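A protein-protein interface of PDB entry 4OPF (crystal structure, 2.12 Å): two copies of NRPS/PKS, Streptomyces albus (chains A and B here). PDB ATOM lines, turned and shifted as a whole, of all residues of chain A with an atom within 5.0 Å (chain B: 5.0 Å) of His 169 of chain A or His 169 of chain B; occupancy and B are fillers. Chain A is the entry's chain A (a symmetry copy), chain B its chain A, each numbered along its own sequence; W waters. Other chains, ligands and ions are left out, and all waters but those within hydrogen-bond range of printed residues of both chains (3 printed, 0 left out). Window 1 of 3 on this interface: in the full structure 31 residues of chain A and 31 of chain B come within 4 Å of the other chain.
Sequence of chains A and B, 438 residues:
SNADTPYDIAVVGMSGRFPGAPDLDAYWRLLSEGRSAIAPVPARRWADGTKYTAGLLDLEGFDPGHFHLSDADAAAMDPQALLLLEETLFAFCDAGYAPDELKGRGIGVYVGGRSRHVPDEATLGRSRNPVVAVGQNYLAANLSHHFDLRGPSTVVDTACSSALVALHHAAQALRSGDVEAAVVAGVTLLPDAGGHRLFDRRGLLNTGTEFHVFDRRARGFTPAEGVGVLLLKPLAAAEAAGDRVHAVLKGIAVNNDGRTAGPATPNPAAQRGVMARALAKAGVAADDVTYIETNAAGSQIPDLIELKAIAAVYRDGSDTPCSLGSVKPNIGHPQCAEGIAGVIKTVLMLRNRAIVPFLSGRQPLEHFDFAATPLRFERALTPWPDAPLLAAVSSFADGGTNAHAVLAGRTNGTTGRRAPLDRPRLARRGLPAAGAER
His 169 of chain A touches just one residue of chain B: His 169 (3.9 Å).
Of the printed residues of chain A, Gln 172 of chain B touches Gln 172 (3.5 Å) and Ala 173 (3.4 Å).
Of the printed residues of chain B, Gln 172 of chain A touches Gln 172 (3.5 Å) and Ala 173 (3.4 Å).
Printed residues of chain A within 4 Å of Ala 173 of chain B: Gln 172 (3.4 Å).
Of the printed residues of chain B, Ala 173 of chain A touches Gln 172 (3.4 Å).
Leu 167 of chain A touches none of the printed residues of chain B.
Val 165 of chain B touches none of the printed residues of chain A.
The nearest residue of chain B that does not touch His 169 of chain A is Thr 154 of chain B (4.2 Å).
His 169 of chain B touches its own counterpart, His 169 of chain A.
Gln 172 of chain A touches its own counterpart, Gln 172 of chain B.
Gln 172 of chain A touches Ala 173 of chain B, and with the chains exchanged Ala 173 of chain A touches Gln 172 of chain B.
Positions printed for both chains: 110, 154, 156, 165, 166, 167, 168, 169, 170, 171, 172 and 173.
Of the 4 pairs that touch across the chains among the printed residues, 4 have their exchanged pair printed and touching as well.
The side-chain amide oxygen of Gln 172 of chain B lies close to the backbone NH of Ala 173 of chain A (3.4 Å).
The backbone NH (N) of Ala 173 of chain B sits close to the side-chain amide oxygen (OE1) of Gln 172 of chain A, 3.4 Å away.
Among the printed residues, pairs that only touch across the chains: His 169 of chain A with His 169 of chain B (3.9 Å) and Gln 172 of chain A with Gln 172 of chain B (3.5 Å).
Printed residues of chain A that touch a printed residue of chain B: His 169, Gln 172 and Ala 173.
Hydrophobic or aromatic side chains of chain A within 4 Å of the printed part of chain B: His 169 and Ala 173.
Along chain A the printed residues that touch a printed residue of chain B span positions 169 to 173.
Hydrophobic or aromatic side chains of chain B that line the printed part of chain A: His 169 and Ala 173.
Water W3 bridges OE1 of Gln 172 of chain A (2.8 Å) and O of His 169 of chain B (2.8 Å).
Water W2 bridges the side-chain amide oxygen of Gln 172 of chain B (2.8 Å) and the backbone carbonyl oxygen of His 169 of chain A (2.8 Å).
Water W1 lies within hydrogen-bond range of ND1 of His 169 of chain B and ND1 of His 169 of chain A.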
ATOM      1  N   TYR A 110     -20.579  21.297   5.023  1.00  0.00           N
ATOM      2  CA  TYR A 110     -19.963  20.793   3.819  1.00  0.00           C
ATOM      3  C   TYR A 110     -21.017  20.085   3.014  1.00  0.00           C
ATOM      4  O   TYR A 110     -21.538  19.051   3.453  1.00  0.00           O
ATOM      5  CB  TYR A 110     -18.822  19.821   4.185  1.00  0.00           C
ATOM      6  CG  TYR A 110     -17.790  20.494   5.069  1.00  0.00           C
ATOM      7  CD1 TYR A 110     -16.767  21.260   4.540  1.00  0.00           C
ATOM      8  CD2 TYR A 110     -17.939  20.495   6.427  1.00  0.00           C
ATOM      9  CE1 TYR A 110     -15.838  21.904   5.373  1.00  0.00           C
ATOM     10  CE2 TYR A 110     -17.027  21.119   7.249  1.00  0.00           C
ATOM     11  CZ  TYR A 110     -15.992  21.830   6.718  1.00  0.00           C
ATOM     12  OH  TYR A 110     -15.106  22.473   7.570  1.00  0.00           O
ATOM     13  N   THR A 154     -19.042  25.328   2.923  1.00  0.00           N
ATOM     14  CA  THR A 154     -18.608  25.093   1.555  1.00  0.00           C
ATOM     15  C   THR A 154     -19.453  24.081   0.810  1.00  0.00           C
ATOM     16  O   THR A 154     -19.988  23.128   1.376  1.00  0.00           O
ATOM     17  CB  THR A 154     -17.112  24.613   1.493  1.00  0.00           C
ATOM     18  OG1 THR A 154     -16.931  23.519   2.332  1.00  0.00           O
ATOM     19  CG2 THR A 154     -16.136  25.669   2.019  1.00  0.00           C
ATOM     20  N   VAL A 156     -19.398  21.580  -2.642  1.00  0.00           N
ATOM     21  CA  VAL A 156     -18.613  20.956  -3.691  1.00  0.00           C
ATOM     22  C   VAL A 156     -19.482  20.252  -4.692  1.00  0.00           C
ATOM     23  O   VAL A 156     -20.460  19.598  -4.347  1.00  0.00           O
ATOM     24  CB  VAL A 156     -17.534  20.006  -3.135  1.00  0.00           C
ATOM     25  CG1 VAL A 156     -16.514  20.825  -2.370  1.00  0.00           C
ATOM     26  CG2 VAL A 156     -18.101  19.010  -2.187  1.00  0.00           C
ATOM     27  N   VAL A 165     -16.632  13.754  -1.146  1.00  0.00           N
ATOM     28  CA  VAL A 165     -15.629  14.821  -1.118  1.00  0.00           C
ATOM     29  C   VAL A 165     -15.943  15.809  -0.014  1.00  0.00           C
ATOM     30  O   VAL A 165     -15.054  16.274   0.713  1.00  0.00           O
ATOM     31  CB  VAL A 165     -15.549  15.509  -2.492  1.00  0.00           C
ATOM     32  CG1 VAL A 165     -14.643  16.700  -2.456  1.00  0.00           C
ATOM     33  CG2 VAL A 165     -15.047  14.505  -3.512  1.00  0.00           C
ATOM     34  N   ALA A 166     -17.236  16.125   0.157  1.00  0.00           N
ATOM     35  CA  ALA A 166     -17.650  17.007   1.296  1.00  0.00           C
ATOM     36  C   ALA A 166     -17.287  16.342   2.632  1.00  0.00           C
ATOM     37  O   ALA A 166     -16.770  16.966   3.545  1.00  0.00           O
ATOM     38  CB  ALA A 166     -19.186  17.264   1.230  1.00  0.00           C
ATOM     39  N   LEU A 167     -17.534  15.046   2.739  1.00  0.00           N
ATOM     40  CA  LEU A 167     -17.107  14.280   3.943  1.00  0.00           C
ATOM     41  C   LEU A 167     -15.573  14.352   4.251  1.00  0.00           C
ATOM     42  O   LEU A 167     -15.140  14.498   5.387  1.00  0.00           O
ATOM     43  CB  LEU A 167     -17.596  12.811   3.809  1.00  0.00           C
ATOM     44  CG  LEU A 167     -17.315  11.936   5.027  1.00  0.00           C
ATOM     45  CD1 LEU A 167     -18.026  12.462   6.246  1.00  0.00           C
ATOM     46  CD2 LEU A 167     -17.804  10.518   4.745  1.00  0.00           C
ATOM     47  N   HIS A 168     -14.771  14.317   3.203  1.00  0.00           N
ATOM     48  CA  HIS A 168     -13.345  14.454   3.295  1.00  0.00           C
ATOM     49  C   HIS A 168     -12.973  15.868   3.783  1.00  0.00           C
ATOM     50  O   HIS A 168     -12.097  15.997   4.638  1.00  0.00           O
ATOM     51  CB  HIS A 168     -12.769  14.189   1.924  1.00  0.00           C
ATOM     52  CG  HIS A 168     -11.291  14.277   1.851  1.00  0.00           C
ATOM     53  ND1 HIS A 168     -10.644  15.204   1.069  1.00  0.00           N
ATOM     54  CD2 HIS A 168     -10.321  13.603   2.515  1.00  0.00           C
ATOM     55  CE1 HIS A 168      -9.341  15.058   1.192  1.00  0.00           C
ATOM     56  NE2 HIS A 168      -9.118  14.104   2.082  1.00  0.00           N
ATOM     57  N   HIS A 169     -13.611  16.911   3.252  1.00  0.00           N
ATOM     58  CA  HIS A 169     -13.296  18.288   3.764  1.00  0.00           C
ATOM     59  C   HIS A 169     -13.693  18.341   5.240  1.00  0.00           C
ATOM     60  O   HIS A 169     -12.966  18.830   6.038  1.00  0.00           O
ATOM     61  CB  HIS A 169     -14.109  19.325   3.021  1.00  0.00           C
ATOM     62  CG  HIS A 169     -13.711  19.531   1.603  1.00  0.00           C
ATOM     63  ND1 HIS A 169     -12.403  19.499   1.171  1.00  0.00           N
ATOM     64  CD2 HIS A 169     -14.452  19.808   0.514  1.00  0.00           C
ATOM     65  CE1 HIS A 169     -12.364  19.696  -0.137  1.00  0.00           C
ATOM     66  NE2 HIS A 169     -13.595  19.873  -0.560  1.00  0.00           N
ATOM     67  N   ALA A 170     -14.818  17.722   5.625  1.00  0.00           N
ATOM     68  CA  ALA A 170     -15.211  17.763   7.011  1.00  0.00           C
ATOM     69  C   ALA A 170     -14.193  17.036   7.900  1.00  0.00           C
ATOM     70  O   ALA A 170     -13.797  17.548   8.971  1.00  0.00           O
ATOM     71  CB  ALA A 170     -16.568  17.165   7.208  1.00  0.00           C
ATOM     72  N   ALA A 171     -13.786  15.856   7.491  1.00  0.00           N
ATOM     73  CA  ALA A 171     -12.799  15.079   8.287  1.00  0.00           C
ATOM     74  C   ALA A 171     -11.471  15.828   8.434  1.00  0.00           C
ATOM     75  O   ALA A 171     -10.886  15.844   9.513  1.00  0.00           O
ATOM     76  CB  ALA A 171     -12.547  13.754   7.612  1.00  0.00           C
ATOM     77  N   GLN A 172     -11.006  16.463   7.368  1.00  0.00           N
ATOM     78  CA  GLN A 172      -9.775  17.268   7.482  1.00  0.00           C
ATOM     79  C   GLN A 172      -9.980  18.394   8.458  1.00  0.00           C
ATOM     80  O   GLN A 172      -9.116  18.681   9.277  1.00  0.00           O
ATOM     81  CB  GLN A 172      -9.395  17.864   6.162  1.00  0.00           C
ATOM     82  CG  GLN A 172      -9.344  16.885   4.996  1.00  0.00           C
ATOM     83  CD  GLN A 172      -7.978  16.640   4.466  1.00  0.00           C
ATOM     84  OE1 GLN A 172      -7.442  17.452   3.727  1.00  0.00           O
ATOM     85  NE2 GLN A 172      -7.397  15.492   4.822  1.00  0.00           N
ATOM     86  N   ALA A 173     -11.172  19.028   8.423  1.00  0.00           N
ATOM     87  CA  ALA A 173     -11.399  20.124   9.322  1.00  0.00           C
ATOM     88  C   ALA A 173     -11.444  19.658  10.762  1.00  0.00           C
ATOM     89  O   ALA A 173     -10.942  20.330  11.697  1.00  0.00           O
ATOM     90  CB  ALA A 173     -12.676  20.879   8.926  1.00  0.00           C
ATOM     91  N   TYR B 110      -6.507  23.192  -6.247  1.00  0.00           N
ATOM     92  CA  TYR B 110      -7.516  23.903  -5.498  1.00  0.00           C
ATOM     93  C   TYR B 110      -7.692  25.259  -6.121  1.00  0.00           C
ATOM     94  O   TYR B 110      -6.765  26.079  -6.089  1.00  0.00           O
ATOM     95  CB  TYR B 110      -7.073  24.041  -4.027  1.00  0.00           C
ATOM     96  CG  TYR B 110      -6.806  22.683  -3.405  1.00  0.00           C
ATOM     97  CD1 TYR B 110      -7.825  21.915  -2.871  1.00  0.00           C
ATOM     98  CD2 TYR B 110      -5.571  22.109  -3.502  1.00  0.00           C
ATOM     99  CE1 TYR B 110      -7.568  20.646  -2.328  1.00  0.00           C
ATOM    100  CE2 TYR B 110      -5.311  20.867  -2.964  1.00  0.00           C
ATOM    101  CZ  TYR B 110      -6.313  20.139  -2.394  1.00  0.00           C
ATOM    102  OH  TYR B 110      -6.028  18.880  -1.889  1.00  0.00           O
ATOM    103  N   THR B 154     -10.349  20.375  -6.820  1.00  0.00           N
ATOM    104  CA  THR B 154     -11.568  21.023  -6.362  1.00  0.00           C
ATOM    105  C   THR B 154     -11.620  22.507  -6.657  1.00  0.00           C
ATOM    106  O   THR B 154     -10.609  23.210  -6.673  1.00  0.00           O
ATOM    107  CB  THR B 154     -11.785  20.830  -4.818  1.00  0.00           C
ATOM    108  OG1 THR B 154     -10.646  21.230  -4.126  1.00  0.00           O
ATOM    109  CG2 THR B 154     -11.977  19.360  -4.432  1.00  0.00           C
ATOM    110  N   VAL B 156     -13.680  26.066  -5.533  1.00  0.00           N
ATOM    111  CA  VAL B 156     -14.543  26.731  -4.575  1.00  0.00           C
ATOM    112  C   VAL B 156     -14.941  28.103  -5.041  1.00  0.00           C
ATOM    113  O   VAL B 156     -14.140  28.850  -5.592  1.00  0.00           O
ATOM    114  CB  VAL B 156     -13.928  26.788  -3.164  1.00  0.00           C
ATOM    115  CG1 VAL B 156     -13.822  25.376  -2.624  1.00  0.00           C
ATOM    116  CG2 VAL B 156     -12.555  27.359  -3.178  1.00  0.00           C
ATOM    117  N   VAL B 165      -9.870  30.427   0.599  1.00  0.00           N
ATOM    118  CA  VAL B 165     -10.514  29.170   0.989  1.00  0.00           C
ATOM    119  C   VAL B 165      -9.860  28.003   0.279  1.00  0.00           C
ATOM    120  O   VAL B 165      -9.613  26.940   0.869  1.00  0.00           O
ATOM    121  CB  VAL B 165     -12.023  29.235   0.704  1.00  0.00           C
ATOM    122  CG1 VAL B 165     -12.686  27.916   0.951  1.00  0.00           C
ATOM    123  CG2 VAL B 165     -12.641  30.301   1.589  1.00  0.00           C
ATOM    124  N   ALA B 166      -9.528  28.195  -1.006  1.00  0.00           N
ATOM    125  CA  ALA B 166      -8.776  27.134  -1.754  1.00  0.00           C
ATOM    126  C   ALA B 166      -7.413  26.890  -1.089  1.00  0.00           C
ATOM    127  O   ALA B 166      -6.979  25.765  -0.898  1.00  0.00           O
ATOM    128  CB  ALA B 166      -8.572  27.580  -3.234  1.00  0.00           C
ATOM    129  N   LEU B 167      -6.741  27.960  -0.701  1.00  0.00           N
ATOM    130  CA  LEU B 167      -5.469  27.833   0.067  1.00  0.00           C
ATOM    131  C   LEU B 167      -5.589  27.017   1.397  1.00  0.00           C
ATOM    132  O   LEU B 167      -4.746  26.197   1.741  1.00  0.00           O
ATOM    133  CB  LEU B 167      -4.881  29.249   0.314  1.00  0.00           C
ATOM    134  CG  LEU B 167      -3.519  29.258   1.002  1.00  0.00           C
ATOM    135  CD1 LEU B 167      -2.484  28.561   0.159  1.00  0.00           C
ATOM    136  CD2 LEU B 167      -3.082  30.704   1.224  1.00  0.00           C
ATOM    137  N   HIS B 168      -6.692  27.209   2.096  1.00  0.00           N
ATOM    138  CA  HIS B 168      -7.005  26.486   3.296  1.00  0.00           C
ATOM    139  C   HIS B 168      -7.230  24.995   2.977  1.00  0.00           C
ATOM    140  O   HIS B 168      -6.735  24.142   3.715  1.00  0.00           O
ATOM    141  CB  HIS B 168      -8.248  27.103   3.892  1.00  0.00           C
ATOM    142  CG  HIS B 168      -8.699  26.473   5.157  1.00  0.00           C
ATOM    143  ND1 HIS B 168      -9.917  25.847   5.276  1.00  0.00           N
ATOM    144  CD2 HIS B 168      -8.072  26.306   6.345  1.00  0.00           C
ATOM    145  CE1 HIS B 168     -10.059  25.381   6.500  1.00  0.00           C
ATOM    146  NE2 HIS B 168      -8.942  25.629   7.165  1.00  0.00           N
ATOM    147  N   HIS B 169      -7.966  24.676   1.914  1.00  0.00           N
ATOM    148  CA  HIS B 169      -8.143  23.225   1.564  1.00  0.00           C
ATOM    149  C   HIS B 169      -6.764  22.655   1.226  1.00  0.00           C
ATOM    150  O   HIS B 169      -6.428  21.605   1.662  1.00  0.00           O
ATOM    151  CB  HIS B 169      -9.022  23.079   0.343  1.00  0.00           C
ATOM    152  CG  HIS B 169     -10.454  23.420   0.562  1.00  0.00           C
ATOM    153  ND1 HIS B 169     -11.135  23.120   1.722  1.00  0.00           N
ATOM    154  CD2 HIS B 169     -11.353  24.006  -0.252  1.00  0.00           C
ATOM    155  CE1 HIS B 169     -12.379  23.558   1.631  1.00  0.00           C
ATOM    156  NE2 HIS B 169     -12.532  24.110   0.449  1.00  0.00           N
ATOM    157  N   ALA B 170      -5.908  23.415   0.529  1.00  0.00           N
ATOM    158  CA  ALA B 170      -4.604  22.896   0.199  1.00  0.00           C
ATOM    159  C   ALA B 170      -3.769  22.645   1.461  1.00  0.00           C
ATOM    160  O   ALA B 170      -3.121  21.583   1.601  1.00  0.00           O
ATOM    161  CB  ALA B 170      -3.867  23.820  -0.718  1.00  0.00           C
ATOM    162  N   ALA B 171      -3.753  23.602   2.361  1.00  0.00           N
ATOM    163  CA  ALA B 171      -2.971  23.448   3.616  1.00  0.00           C
ATOM    164  C   ALA B 171      -3.457  22.255   4.446  1.00  0.00           C
ATOM    165  O   ALA B 171      -2.648  21.506   4.983  1.00  0.00           O
ATOM    166  CB  ALA B 171      -3.096  24.705   4.440  1.00  0.00           C
ATOM    167  N   GLN B 172      -4.766  22.065   4.533  1.00  0.00           N
ATOM    168  CA  GLN B 172      -5.282  20.882   5.251  1.00  0.00           C
ATOM    169  C   GLN B 172      -4.821  19.623   4.569  1.00  0.00           C
ATOM    170  O   GLN B 172      -4.418  18.667   5.222  1.00  0.00           O
ATOM    171  CB  GLN B 172      -6.778  20.874   5.273  1.00  0.00           C
ATOM    172  CG  GLN B 172      -7.428  22.169   5.745  1.00  0.00           C
ATOM    173  CD  GLN B 172      -8.122  22.060   7.054  1.00  0.00           C
ATOM    174  OE1 GLN B 172      -9.229  21.550   7.130  1.00  0.00           O
ATOM    175  NE2 GLN B 172      -7.485  22.568   8.111  1.00  0.00           N
ATOM    176  N   ALA B 173      -4.824  19.617   3.219  1.00  0.00           N
ATOM    177  CA  ALA B 173      -4.415  18.426   2.530  1.00  0.00           C
ATOM    178  C   ALA B 173      -2.943  18.140   2.745  1.00  0.00           C
ATOM    179  O   ALA B 173      -2.505  16.972   2.900  1.00  0.00           O
ATOM    180  CB  ALA B 173      -4.764  18.527   1.039  1.00  0.00           C
HETATM  181  O   HOH W   1     -10.398  20.587   3.037  1.00  0.00           O
HETATM  182  O   HOH W   2     -11.534  21.227   5.524  1.00  0.00           O
HETATM  183  O   HOH W   3      -8.185  19.380   1.798  1.00  0.00           O
